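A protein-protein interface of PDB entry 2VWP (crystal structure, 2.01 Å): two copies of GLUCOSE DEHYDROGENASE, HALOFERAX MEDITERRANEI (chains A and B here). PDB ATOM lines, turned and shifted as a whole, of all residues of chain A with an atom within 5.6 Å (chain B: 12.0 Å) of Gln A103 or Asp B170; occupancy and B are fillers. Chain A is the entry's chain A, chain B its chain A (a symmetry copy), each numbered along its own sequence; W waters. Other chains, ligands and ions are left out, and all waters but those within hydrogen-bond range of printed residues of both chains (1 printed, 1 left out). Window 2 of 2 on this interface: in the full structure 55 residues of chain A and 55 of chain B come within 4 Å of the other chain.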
ATOM      1  N   GLU A  97      23.192   9.769 -15.225  1.00  0.00           N
ATOM      2  CA  GLU A  97      22.039   9.608 -14.315  1.00  0.00           C
ATOM      3  C   GLU A  97      21.792   8.160 -13.861  1.00  0.00           C
ATOM      4  O   GLU A  97      21.397   7.930 -12.724  1.00  0.00           O
ATOM      5  CB  GLU A  97      20.758  10.178 -14.950  1.00  0.00           C
ATOM      6  CG  GLU A  97      20.427   9.576 -16.330  1.00  0.00           C
ATOM      7  CD  GLU A  97      19.036   9.914 -16.848  1.00  0.00           C
ATOM      8  OE1 GLU A  97      18.038   9.619 -16.155  1.00  0.00           O
ATOM      9  OE2 GLU A  97      18.942  10.440 -17.978  1.00  0.00           O
ATOM     10  N   TYR A  98      22.025   7.199 -14.754  1.00  0.00           N
ATOM     11  CA  TYR A  98      21.807   5.776 -14.457  1.00  0.00           C
ATOM     12  C   TYR A  98      22.774   5.285 -13.412  1.00  0.00           C
ATOM     13  O   TYR A  98      22.371   4.618 -12.454  1.00  0.00           O
ATOM     14  CB  TYR A  98      21.913   4.947 -15.732  1.00  0.00           C
ATOM     15  CG  TYR A  98      20.886   5.377 -16.723  1.00  0.00           C
ATOM     16  CD1 TYR A  98      21.241   6.162 -17.815  1.00  0.00           C
ATOM     17  CD2 TYR A  98      19.533   5.044 -16.544  1.00  0.00           C
ATOM     18  CE1 TYR A  98      20.294   6.582 -18.733  1.00  0.00           C
ATOM     19  CE2 TYR A  98      18.577   5.462 -17.455  1.00  0.00           C
ATOM     20  CZ  TYR A  98      18.967   6.232 -18.547  1.00  0.00           C
ATOM     21  OH  TYR A  98      18.038   6.658 -19.467  1.00  0.00           O
ATOM     22  N   PHE A  99      24.042   5.654 -13.584  1.00  0.00           N
ATOM     23  CA  PHE A  99      25.079   5.340 -12.607  1.00  0.00           C
ATOM     24  C   PHE A  99      24.899   6.112 -11.300  1.00  0.00           C
ATOM     25  O   PHE A  99      25.056   5.542 -10.218  1.00  0.00           O
ATOM     26  CB  PHE A  99      26.476   5.508 -13.235  1.00  0.00           C
ATOM     27  CG  PHE A  99      26.811   4.418 -14.228  1.00  0.00           C
ATOM     28  CD1 PHE A  99      27.415   3.232 -13.800  1.00  0.00           C
ATOM     29  CD2 PHE A  99      26.480   4.558 -15.575  1.00  0.00           C
ATOM     30  CE1 PHE A  99      27.695   2.208 -14.702  1.00  0.00           C
ATOM     31  CE2 PHE A  99      26.758   3.546 -16.486  1.00  0.00           C
ATOM     32  CZ  PHE A  99      27.365   2.363 -16.050  1.00  0.00           C
ATOM     33  N   ARG A 101      22.071   7.272 -10.015  1.00  0.00           N
ATOM     34  CA  ARG A 101      20.878   6.767  -9.334  1.00  0.00           C
ATOM     35  C   ARG A 101      20.957   5.288  -8.950  1.00  0.00           C
ATOM     36  O   ARG A 101      19.945   4.703  -8.559  1.00  0.00           O
ATOM     37  CB  ARG A 101      19.633   6.983 -10.198  1.00  0.00           C
ATOM     38  CG  ARG A 101      19.173   8.432 -10.295  1.00  0.00           C
ATOM     39  CD  ARG A 101      17.674   8.500 -10.566  1.00  0.00           C
ATOM     40  NE  ARG A 101      17.325   9.607 -11.456  1.00  0.00           N
ATOM     41  CZ  ARG A 101      16.102   9.839 -11.932  1.00  0.00           C
ATOM     42  NH1 ARG A 101      15.087   9.041 -11.601  1.00  0.00           N
ATOM     43  NH2 ARG A 101      15.890  10.878 -12.739  1.00  0.00           N
ATOM     44  N   ASP A 102      22.149   4.692  -9.064  1.00  0.00           N
ATOM     45  CA  ASP A 102      22.376   3.270  -8.756  1.00  0.00           C
ATOM     46  C   ASP A 102      21.453   2.328  -9.542  1.00  0.00           C
ATOM     47  O   ASP A 102      20.932   1.336  -8.999  1.00  0.00           O
ATOM     48  CB  ASP A 102      22.263   2.997  -7.250  1.00  0.00           C
ATOM     49  CG  ASP A 102      23.191   3.875  -6.416  1.00  0.00           C
ATOM     50  OD1 ASP A 102      24.398   3.970  -6.742  1.00  0.00           O
ATOM     51  OD2 ASP A 102      22.703   4.457  -5.423  1.00  0.00           O
ATOM     52  N   GLN A 103      21.253   2.649 -10.819  1.00  0.00           N
ATOM     53  CA  GLN A 103      20.539   1.748 -11.726  1.00  0.00           C
ATOM     54  C   GLN A 103      21.178   1.699 -13.116  1.00  0.00           C
ATOM     55  O   GLN A 103      20.517   1.971 -14.107  1.00  0.00           O
ATOM     56  CB  GLN A 103      19.020   2.070 -11.785  1.00  0.00           C
ATOM     57  CG  GLN A 103      18.649   3.509 -12.167  1.00  0.00           C
ATOM     58  CD  GLN A 103      17.125   3.800 -12.139  1.00  0.00           C
ATOM     59  OE1 GLN A 103      16.404   3.373 -11.225  1.00  0.00           O
ATOM     60  NE2 GLN A 103      16.644   4.548 -13.145  1.00  0.00           N
ATOM     61  N   PRO A 104      22.485   1.350 -13.199  1.00  0.00           N
ATOM     62  CA  PRO A 104      23.124   1.282 -14.519  1.00  0.00           C
ATOM     63  C   PRO A 104      22.574   0.163 -15.429  1.00  0.00           C
ATOM     64  O   PRO A 104      22.737   0.212 -16.638  1.00  0.00           O
ATOM     65  CB  PRO A 104      24.605   1.047 -14.180  1.00  0.00           C
ATOM     66  CG  PRO A 104      24.608   0.459 -12.848  1.00  0.00           C
ATOM     67  CD  PRO A 104      23.426   0.996 -12.119  1.00  0.00           C
ATOM     68  N   ASP A 105      21.913  -0.823 -14.829  1.00  0.00           N
ATOM     69  CA  ASP A 105      21.237  -1.897 -15.554  1.00  0.00           C
ATOM     70  C   ASP A 105      20.121  -1.392 -16.483  1.00  0.00           C
ATOM     71  O   ASP A 105      19.725  -2.091 -17.410  1.00  0.00           O
ATOM     72  CB  ASP A 105      20.691  -2.916 -14.541  1.00  0.00           C
ATOM     73  CG  ASP A 105      19.683  -2.301 -13.578  1.00  0.00           C
ATOM     74  OD1 ASP A 105      20.069  -1.538 -12.667  1.00  0.00           O
ATOM     75  OD2 ASP A 105      18.494  -2.597 -13.737  1.00  0.00           O
ATOM     76  N   MET A 106      19.649  -0.163 -16.240  1.00  0.00           N
ATOM     77  CA  MET A 106      18.607   0.475 -17.032  1.00  0.00           C
ATOM     78  C   MET A 106      19.203   1.467 -18.031  1.00  0.00           C
ATOM     79  O   MET A 106      18.469   2.068 -18.813  1.00  0.00           O
ATOM     80  CB  MET A 106      17.599   1.209 -16.102  1.00  0.00           C
ATOM     81  CG  MET A 106      16.947   0.332 -15.002  1.00  0.00           C
ATOM     82  SD  MET A 106      16.048  -1.112 -15.623  1.00  0.00           S
ATOM     83  CE  MET A 106      14.762  -0.320 -16.588  1.00  0.00           C
ATOM     84  N   ALA A 107      20.529   1.657 -17.990  1.00  0.00           N
ATOM     85  CA  ALA A 107      21.221   2.499 -18.983  1.00  0.00           C
ATOM     86  C   ALA A 107      21.041   1.936 -20.376  1.00  0.00           C
ATOM     87  O   ALA A 107      21.161   0.730 -20.568  1.00  0.00           O
ATOM     88  CB  ALA A 107      22.730   2.638 -18.657  1.00  0.00           C
ATOM     89  N   HIS A 305      21.711  -5.444 -11.095  1.00  0.00           N
ATOM     90  CA  HIS A 305      22.498  -4.631 -10.181  1.00  0.00           C
ATOM     91  C   HIS A 305      22.563  -5.212  -8.777  1.00  0.00           C
ATOM     92  O   HIS A 305      22.146  -6.354  -8.551  1.00  0.00           O
ATOM     93  CB  HIS A 305      22.047  -3.158 -10.189  1.00  0.00           C
ATOM     94  CG  HIS A 305      23.143  -2.199  -9.830  1.00  0.00           C
ATOM     95  ND1 HIS A 305      24.397  -2.248 -10.412  1.00  0.00           N
ATOM     96  CD2 HIS A 305      23.181  -1.178  -8.944  1.00  0.00           C
ATOM     97  CE1 HIS A 305      25.158  -1.301  -9.896  1.00  0.00           C
ATOM     98  NE2 HIS A 305      24.444  -0.636  -9.005  1.00  0.00           N
ATOM     99  N   ALA B 162       0.121  -0.125 -16.785  1.00  0.00           N
ATOM    100  CA  ALA B 162       1.330   0.302 -17.489  1.00  0.00           C
ATOM    101  C   ALA B 162       2.384   0.855 -16.514  1.00  0.00           C
ATOM    102  O   ALA B 162       3.561   0.474 -16.581  1.00  0.00           O
ATOM    103  CB  ALA B 162       1.010   1.312 -18.573  1.00  0.00           C
ATOM    104  N   TYR B 163       1.950   1.720 -15.595  1.00  0.00           N
ATOM    105  CA  TYR B 163       2.847   2.292 -14.585  1.00  0.00           C
ATOM    106  C   TYR B 163       3.393   1.235 -13.607  1.00  0.00           C
ATOM    107  O   TYR B 163       4.575   1.282 -13.217  1.00  0.00           O
ATOM    108  CB  TYR B 163       2.171   3.451 -13.834  1.00  0.00           C
ATOM    109  CG  TYR B 163       1.830   4.677 -14.686  1.00  0.00           C
ATOM    110  CD1 TYR B 163       2.333   4.825 -15.999  1.00  0.00           C
ATOM    111  CD2 TYR B 163       1.013   5.691 -14.177  1.00  0.00           C
ATOM    112  CE1 TYR B 163       2.036   5.948 -16.764  1.00  0.00           C
ATOM    113  CE2 TYR B 163       0.704   6.827 -14.945  1.00  0.00           C
ATOM    114  CZ  TYR B 163       1.222   6.951 -16.225  1.00  0.00           C
ATOM    115  OH  TYR B 163       0.931   8.067 -16.976  1.00  0.00           O
ATOM    116  N   ALA B 164       2.535   0.283 -13.228  1.00  0.00           N
ATOM    117  CA  ALA B 164       2.955  -0.861 -12.420  1.00  0.00           C
ATOM    118  C   ALA B 164       4.129  -1.600 -13.075  1.00  0.00           C
ATOM    119  O   ALA B 164       5.068  -2.014 -12.372  1.00  0.00           O
ATOM    120  CB  ALA B 164       1.773  -1.828 -12.129  1.00  0.00           C
ATOM    121  N   SER B 165       4.111  -1.721 -14.407  1.00  0.00           N
ATOM    122  CA  SER B 165       5.210  -2.382 -15.127  1.00  0.00           C
ATOM    123  C   SER B 165       6.561  -1.697 -14.895  1.00  0.00           C
ATOM    124  O   SER B 165       7.610  -2.354 -14.954  1.00  0.00           O
ATOM    125  CB  SER B 165       4.911  -2.565 -16.640  1.00  0.00           C
ATOM    126  OG  SER B 165       5.285  -1.430 -17.408  1.00  0.00           O
ATOM    127  N   ARG B 166       6.521  -0.397 -14.607  1.00  0.00           N
ATOM    128  CA  ARG B 166       7.731   0.415 -14.457  1.00  0.00           C
ATOM    129  C   ARG B 166       8.133   0.627 -12.996  1.00  0.00           C
ATOM    130  O   ARG B 166       9.061   1.381 -12.708  1.00  0.00           O
ATOM    131  CB  ARG B 166       7.547   1.785 -15.153  1.00  0.00           C
ATOM    132  CG  ARG B 166       7.089   1.756 -16.619  1.00  0.00           C
ATOM    133  CD  ARG B 166       8.130   1.170 -17.575  1.00  0.00           C
ATOM    134  NE  ARG B 166       8.185  -0.294 -17.458  1.00  0.00           N
ATOM    135  CZ  ARG B 166       9.211  -1.056 -17.833  1.00  0.00           C
ATOM    136  NH1 ARG B 166       9.153  -2.374 -17.655  1.00  0.00           N
ATOM    137  NH2 ARG B 166      10.296  -0.511 -18.386  1.00  0.00           N
ATOM    138  N   SER B 167       7.447  -0.048 -12.079  1.00  0.00           N
ATOM    139  CA  SER B 167       7.584   0.257 -10.649  1.00  0.00           C
ATOM    140  C   SER B 167       8.817  -0.350  -9.943  1.00  0.00           C
ATOM    141  O   SER B 167       9.097   0.003  -8.804  1.00  0.00           O
ATOM    142  CB  SER B 167       6.292  -0.086  -9.894  1.00  0.00           C
ATOM    143  OG  SER B 167       6.012  -1.473  -9.974  1.00  0.00           O
ATOM    144  N   ALA B 168       9.554  -1.229 -10.621  1.00  0.00           N
ATOM    145  CA  ALA B 168      10.791  -1.789 -10.051  1.00  0.00           C
ATOM    146  C   ALA B 168      12.010  -0.828 -10.112  1.00  0.00           C
ATOM    147  O   ALA B 168      13.067  -1.106  -9.539  1.00  0.00           O
ATOM    148  CB  ALA B 168      11.122  -3.134 -10.694  1.00  0.00           C
ATOM    149  N   PHE B 169      11.868   0.297 -10.800  1.00  0.00           N
ATOM    150  CA  PHE B 169      12.970   1.261 -10.876  1.00  0.00           C
ATOM    151  C   PHE B 169      12.415   2.672 -10.758  1.00  0.00           C
ATOM    152  O   PHE B 169      11.202   2.857 -10.826  1.00  0.00           O
ATOM    153  CB  PHE B 169      13.822   1.046 -12.152  1.00  0.00           C
ATOM    154  CG  PHE B 169      13.125   1.404 -13.457  1.00  0.00           C
ATOM    155  CD1 PHE B 169      12.143   0.578 -14.007  1.00  0.00           C
ATOM    156  CD2 PHE B 169      13.475   2.550 -14.142  1.00  0.00           C
ATOM    157  CE1 PHE B 169      11.522   0.914 -15.213  1.00  0.00           C
ATOM    158  CE2 PHE B 169      12.859   2.897 -15.332  1.00  0.00           C
ATOM    159  CZ  PHE B 169      11.877   2.064 -15.872  1.00  0.00           C
ATOM    160  N   ASP B 170      13.285   3.662 -10.566  1.00  0.00           N
ATOM    161  CA  ASP B 170      12.860   5.065 -10.554  1.00  0.00           C
ATOM    162  C   ASP B 170      12.667   5.595 -11.983  1.00  0.00           C
ATOM    163  O   ASP B 170      13.570   6.178 -12.590  1.00  0.00           O
ATOM    164  CB  ASP B 170      13.829   5.935  -9.725  1.00  0.00           C
ATOM    165  CG  ASP B 170      13.718   5.680  -8.198  1.00  0.00           C
ATOM    166  OD1 ASP B 170      12.666   5.176  -7.705  1.00  0.00           O
ATOM    167  OD2 ASP B 170      14.698   5.995  -7.472  1.00  0.00           O
ATOM    168  N   TRP B 171      11.480   5.349 -12.528  1.00  0.00           N
ATOM    169  CA  TRP B 171      11.116   5.773 -13.871  1.00  0.00           C
ATOM    170  C   TRP B 171      10.731   7.238 -13.831  1.00  0.00           C
ATOM    171  O   TRP B 171       9.917   7.653 -13.013  1.00  0.00           O
ATOM    172  CB  TRP B 171       9.923   4.951 -14.347  1.00  0.00           C
ATOM    173  CG  TRP B 171       9.507   5.152 -15.765  1.00  0.00           C
ATOM    174  CD1 TRP B 171      10.323   5.188 -16.874  1.00  0.00           C
ATOM    175  CD2 TRP B 171       8.160   5.298 -16.252  1.00  0.00           C
ATOM    176  NE1 TRP B 171       9.568   5.356 -18.006  1.00  0.00           N
ATOM    177  CE2 TRP B 171       8.239   5.425 -17.659  1.00  0.00           C
ATOM    178  CE3 TRP B 171       6.896   5.338 -15.634  1.00  0.00           C
ATOM    179  CZ2 TRP B 171       7.097   5.581 -18.470  1.00  0.00           C
ATOM    180  CZ3 TRP B 171       5.760   5.502 -16.435  1.00  0.00           C
ATOM    181  CH2 TRP B 171       5.871   5.621 -17.838  1.00  0.00           C
ATOM    182  N   ASP B 172      11.294   8.013 -14.740  1.00  0.00           N
ATOM    183  CA  ASP B 172      11.118   9.459 -14.723  1.00  0.00           C
ATOM    184  C   ASP B 172      10.739   9.894 -16.132  1.00  0.00           C
ATOM    185  O   ASP B 172      11.573  10.454 -16.861  1.00  0.00           O
ATOM    186  CB  ASP B 172      12.432  10.122 -14.271  1.00  0.00           C
ATOM    187  CG  ASP B 172      12.289  11.616 -13.969  1.00  0.00           C
ATOM    188  OD1 ASP B 172      11.149  12.111 -13.768  1.00  0.00           O
ATOM    189  OD2 ASP B 172      13.350  12.288 -13.912  1.00  0.00           O
ATOM    190  N   PRO B 173       9.481   9.622 -16.535  1.00  0.00           N
ATOM    191  CA  PRO B 173       9.122   9.921 -17.915  1.00  0.00           C
ATOM    192  C   PRO B 173       8.954  11.432 -18.137  1.00  0.00           C
ATOM    193  O   PRO B 173       8.570  12.158 -17.212  1.00  0.00           O
ATOM    194  CB  PRO B 173       7.791   9.207 -18.083  1.00  0.00           C
ATOM    195  CG  PRO B 173       7.197   9.224 -16.714  1.00  0.00           C
ATOM    196  CD  PRO B 173       8.347   9.056 -15.778  1.00  0.00           C
ATOM    197  N   SER B 174       9.233  11.888 -19.353  1.00  0.00           N
ATOM    198  CA  SER B 174       8.992  13.281 -19.704  1.00  0.00           C
ATOM    199  C   SER B 174       8.071  13.421 -20.914  1.00  0.00           C
ATOM    200  O   SER B 174       7.414  14.446 -21.070  1.00  0.00           O
ATOM    201  CB  SER B 174      10.315  14.025 -19.906  1.00  0.00           C
ATOM    202  OG  SER B 174      10.952  13.593 -21.097  1.00  0.00           O
ATOM    203  N   LYS B 197       2.857  12.273 -13.166  1.00  0.00           N
ATOM    204  CA  LYS B 197       4.163  11.967 -13.762  1.00  0.00           C
ATOM    205  C   LYS B 197       4.809  13.237 -14.299  1.00  0.00           C
ATOM    206  O   LYS B 197       5.977  13.220 -14.675  1.00  0.00           O
ATOM    207  CB  LYS B 197       4.045  10.943 -14.907  1.00  0.00           C
ATOM    208  CG  LYS B 197       3.609   9.531 -14.513  1.00  0.00           C
ATOM    209  CD  LYS B 197       4.756   8.668 -14.063  1.00  0.00           C
ATOM    210  CE  LYS B 197       4.289   7.300 -13.604  1.00  0.00           C
ATOM    211  NZ  LYS B 197       3.623   7.354 -12.289  1.00  0.00           N
ATOM    212  N   TYR B 199       4.340  15.074 -17.278  1.00  0.00           N
ATOM    213  CA  TYR B 199       4.865  14.990 -18.652  1.00  0.00           C
ATOM    214  C   TYR B 199       5.153  16.389 -19.215  1.00  0.00           C
ATOM    215  O   TYR B 199       4.342  17.304 -19.054  1.00  0.00           O
ATOM    216  CB  TYR B 199       3.895  14.236 -19.584  1.00  0.00           C
ATOM    217  CG  TYR B 199       3.705  12.769 -19.248  1.00  0.00           C
ATOM    218  CD1 TYR B 199       4.657  11.811 -19.647  1.00  0.00           C
ATOM    219  CD2 TYR B 199       2.581  12.324 -18.537  1.00  0.00           C
ATOM    220  CE1 TYR B 199       4.488  10.445 -19.353  1.00  0.00           C
ATOM    221  CE2 TYR B 199       2.416  10.941 -18.223  1.00  0.00           C
ATOM    222  CZ  TYR B 199       3.364  10.023 -18.649  1.00  0.00           C
ATOM    223  OH  TYR B 199       3.234   8.685 -18.343  1.00  0.00           O
ATOM    224  N   ASP B 244       8.630   8.161 -23.728  1.00  0.00           N
ATOM    225  CA  ASP B 244       8.671   7.358 -22.498  1.00  0.00           C
ATOM    226  C   ASP B 244       7.408   6.539 -22.297  1.00  0.00           C
ATOM    227  O   ASP B 244       7.468   5.385 -21.830  1.00  0.00           O
ATOM    228  CB  ASP B 244       8.888   8.232 -21.264  1.00  0.00           C
ATOM    229  CG  ASP B 244      10.200   8.999 -21.307  1.00  0.00           C
ATOM    230  OD1 ASP B 244      11.265   8.347 -21.340  1.00  0.00           O
ATOM    231  OD2 ASP B 244      10.162  10.251 -21.262  1.00  0.00           O
ATOM    232  N   ALA B 264      11.113   5.331 -25.797  1.00  0.00           N
ATOM    233  CA  ALA B 264      12.394   5.602 -25.164  1.00  0.00           C
ATOM    234  C   ALA B 264      12.847   4.377 -24.363  1.00  0.00           C
ATOM    235  O   ALA B 264      12.022   3.522 -23.981  1.00  0.00           O
ATOM    236  CB  ALA B 264      12.312   6.846 -24.271  1.00  0.00           C
ATOM    237  N   PRO B 265      14.167   4.261 -24.129  1.00  0.00           N
ATOM    238  CA  PRO B 265      14.603   3.179 -23.257  1.00  0.00           C
ATOM    239  C   PRO B 265      13.826   3.201 -21.951  1.00  0.00           C
ATOM    240  O   PRO B 265      13.599   4.276 -21.382  1.00  0.00           O
ATOM    241  CB  PRO B 265      16.082   3.509 -23.008  1.00  0.00           C
ATOM    242  CG  PRO B 265      16.487   4.221 -24.315  1.00  0.00           C
ATOM    243  CD  PRO B 265      15.299   5.065 -24.635  1.00  0.00           C
ATOM    244  N   ASN B 266      13.434   2.014 -21.492  1.00  0.00           N
ATOM    245  CA  ASN B 266      12.800   1.833 -20.195  1.00  0.00           C
ATOM    246  C   ASN B 266      11.338   2.292 -20.243  1.00  0.00           C
ATOM    247  O   ASN B 266      10.695   2.388 -19.227  1.00  0.00           O
ATOM    248  CB  ASN B 266      13.582   2.556 -19.069  1.00  0.00           C
ATOM    249  CG  ASN B 266      15.094   2.255 -19.083  1.00  0.00           C
ATOM    250  OD1 ASN B 266      15.514   1.133 -19.331  1.00  0.00           O
ATOM    251  ND2 ASN B 266      15.912   3.278 -18.807  1.00  0.00           N
ATOM    252  N   GLY B 267      10.830   2.564 -21.444  1.00  0.00           N
ATOM    253  CA  GLY B 267       9.462   3.016 -21.622  1.00  0.00           C
ATOM    254  C   GLY B 267       8.454   1.892 -21.633  1.00  0.00           C
ATOM    255  O   GLY B 267       8.819   0.713 -21.672  1.00  0.00           O
ATOM    256  N   VAL B 268       7.174   2.257 -21.580  1.00  0.00           N
ATOM    257  CA  VAL B 268       6.093   1.270 -21.675  1.00  0.00           C
ATOM    258  C   VAL B 268       5.023   1.730 -22.657  1.00  0.00           C
ATOM    259  O   VAL B 268       4.656   2.916 -22.703  1.00  0.00           O
ATOM    260  CB  VAL B 268       5.453   0.935 -20.267  1.00  0.00           C
ATOM    261  CG1 VAL B 268       5.027   2.209 -19.534  1.00  0.00           C
ATOM    262  CG2 VAL B 268       4.269  -0.071 -20.403  1.00  0.00           C
ATOM    263  N   VAL B 292      14.247  -6.085 -25.116  1.00  0.00           N
ATOM    264  CA  VAL B 292      15.185  -6.632 -24.130  1.00  0.00           C
ATOM    265  C   VAL B 292      16.320  -5.670 -23.793  1.00  0.00           C
ATOM    266  O   VAL B 292      16.529  -5.314 -22.610  1.00  0.00           O
ATOM    267  CB  VAL B 292      15.726  -8.019 -24.615  1.00  0.00           C
ATOM    268  CG1 VAL B 292      16.884  -8.519 -23.735  1.00  0.00           C
ATOM    269  CG2 VAL B 292      14.569  -9.028 -24.661  1.00  0.00           C
ATOM    270  N   LEU B 293      17.047  -5.240 -24.821  1.00  0.00           N
ATOM    271  CA  LEU B 293      18.238  -4.403 -24.622  1.00  0.00           C
ATOM    272  C   LEU B 293      17.910  -3.054 -23.991  1.00  0.00           C
ATOM    273  O   LEU B 293      18.758  -2.429 -23.354  1.00  0.00           O
ATOM    274  CB  LEU B 293      18.991  -4.195 -25.944  1.00  0.00           C
ATOM    275  CG  LEU B 293      19.694  -5.432 -26.503  1.00  0.00           C
ATOM    276  CD1 LEU B 293      20.641  -5.037 -27.623  1.00  0.00           C
ATOM    277  CD2 LEU B 293      20.415  -6.203 -25.396  1.00  0.00           C
ATOM    278  N   HIS B 294      16.670  -2.618 -24.163  1.00  0.00           N
ATOM    279  CA  HIS B 294      16.253  -1.333 -23.636  1.00  0.00           C
ATOM    280  C   HIS B 294      15.150  -1.415 -22.576  1.00  0.00           C
ATOM    281  O   HIS B 294      14.454  -0.426 -22.343  1.00  0.00           O
ATOM    282  CB  HIS B 294      15.886  -0.378 -24.786  1.00  0.00           C
ATOM    283  CG  HIS B 294      17.079   0.264 -25.431  1.00  0.00           C
ATOM    284  ND1 HIS B 294      17.104   0.636 -26.757  1.00  0.00           N
ATOM    285  CD2 HIS B 294      18.298   0.586 -24.928  1.00  0.00           C
ATOM    286  CE1 HIS B 294      18.281   1.166 -27.044  1.00  0.00           C
ATOM    287  NE2 HIS B 294      19.023   1.153 -25.948  1.00  0.00           N
ATOM    288  N   ASN B 295      15.014  -2.585 -21.942  1.00  0.00           N
ATOM    289  CA  ASN B 295      14.119  -2.796 -20.781  1.00  0.00           C
ATOM    290  C   ASN B 295      12.739  -2.167 -20.985  1.00  0.00           C
ATOM    291  O   ASN B 295      12.284  -1.389 -20.146  1.00  0.00           O
ATOM    292  CB  ASN B 295      14.717  -2.181 -19.519  1.00  0.00           C
ATOM    293  CG  ASN B 295      16.084  -2.730 -19.171  1.00  0.00           C
ATOM    294  OD1 ASN B 295      16.196  -3.795 -18.570  1.00  0.00           O
ATOM    295  ND2 ASN B 295      17.139  -1.982 -19.525  1.00  0.00           N
HETATM  296  O   HOH W   1      20.733  -1.643 -21.931  1.00  0.00           O
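The backbone carbonyl oxygen (O) of Asp B170 is in hydrogen-bond range of the guanidinium group (NH1) of Arg A101. The guanidinium group of Arg A101 is in salt-bridge range of the side-chain carboxylate of Asp B172, at 3.1 Å. The side-chain amide nitrogen (ND2) of Asn B295 sits at hydrogen-bond distance from the backbone carbonyl oxygen (O) of Asp A105. N of Asp B170 sits at hydrogen-bond distance from OE1 of Gln A103 (3.2 Å). ND2 of Asn B266 lies within hydrogen-bond range of O of Met A106, 2.8 Å away.
The guanidinium group (NH2) of Arg B166 lies within hydrogen-bond range of the backbone carbonyl oxygen (O) of Asn B295 (2.8 Å). The guanidinium group (NH2) of Arg B166 sits at hydrogen-bond distance from the backbone carbonyl oxygen (O) of Asn B266 (3.0 Å). N of Asn B266 sits at hydrogen-bond distance from O of His B294 (2.8 Å). The indole nitrogen (NE1) of Trp B171 lies within hydrogen-bond range of the backbone carbonyl oxygen (O) of Asn B266 (3.4 Å). O of Tyr A98 sits at hydrogen-bond distance from N of Gln A103 (2.8 Å).
Tyr A98 touches Asn B266 (CE2 to ND2, 3.7 Å). Phe B169 touches Gln A103. Phe B169 touches Met A106 (CE1 to CE, 3.7 Å). Asn B295 touches Met A106 (CB to CE, 3.5 Å).
Of chain B, only Phe B169 and Asp B170 come within 4 Å of Gln A103. Asp B170 touches two residues of chain A. No residue of chain B comes within 4 Å of Phe A99. No residue of chain B comes within 4 Å of Pro A104. Asp A105 touches one residue of chain B. No residue of chain B comes within 4 Å of Ala A107. Printed residues of chain A within 4 Å of Asn B295: Asp A105 and Met A106. Of the printed residues of chain A, Asp B172 touches Arg A101. Printed residues of chain A within 4 Å of Asn B266: Tyr A98 and Met A106. Of the printed residues of chain A, Phe B169 touches Gln A103 and Met A106.
Of the 25 printed residues of chain B, 5 touch a printed residue of chain A. Printed residues of chain A that touch a printed residue of chain B: Tyr A98, Arg A101, Gln A103, Asp A105 and Met A106. Hydrophobic or aromatic side chains of chain A within 4 Å of the printed part of chain B: Tyr A98 and Met A106. Among the printed residues, Asp or Glu carboxylates within 4 Å of a Lys or Arg side-chain nitrogen of the other chain: Arg A101 with Asp B172 (3.1 Å).
No position is printed for both chains.
Water W1 bridges the backbone carbonyl oxygen (O) of Leu B293 (2.6 Å) and the backbone carbonyl oxygen (O) of Ala A107 (2.8 Å).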
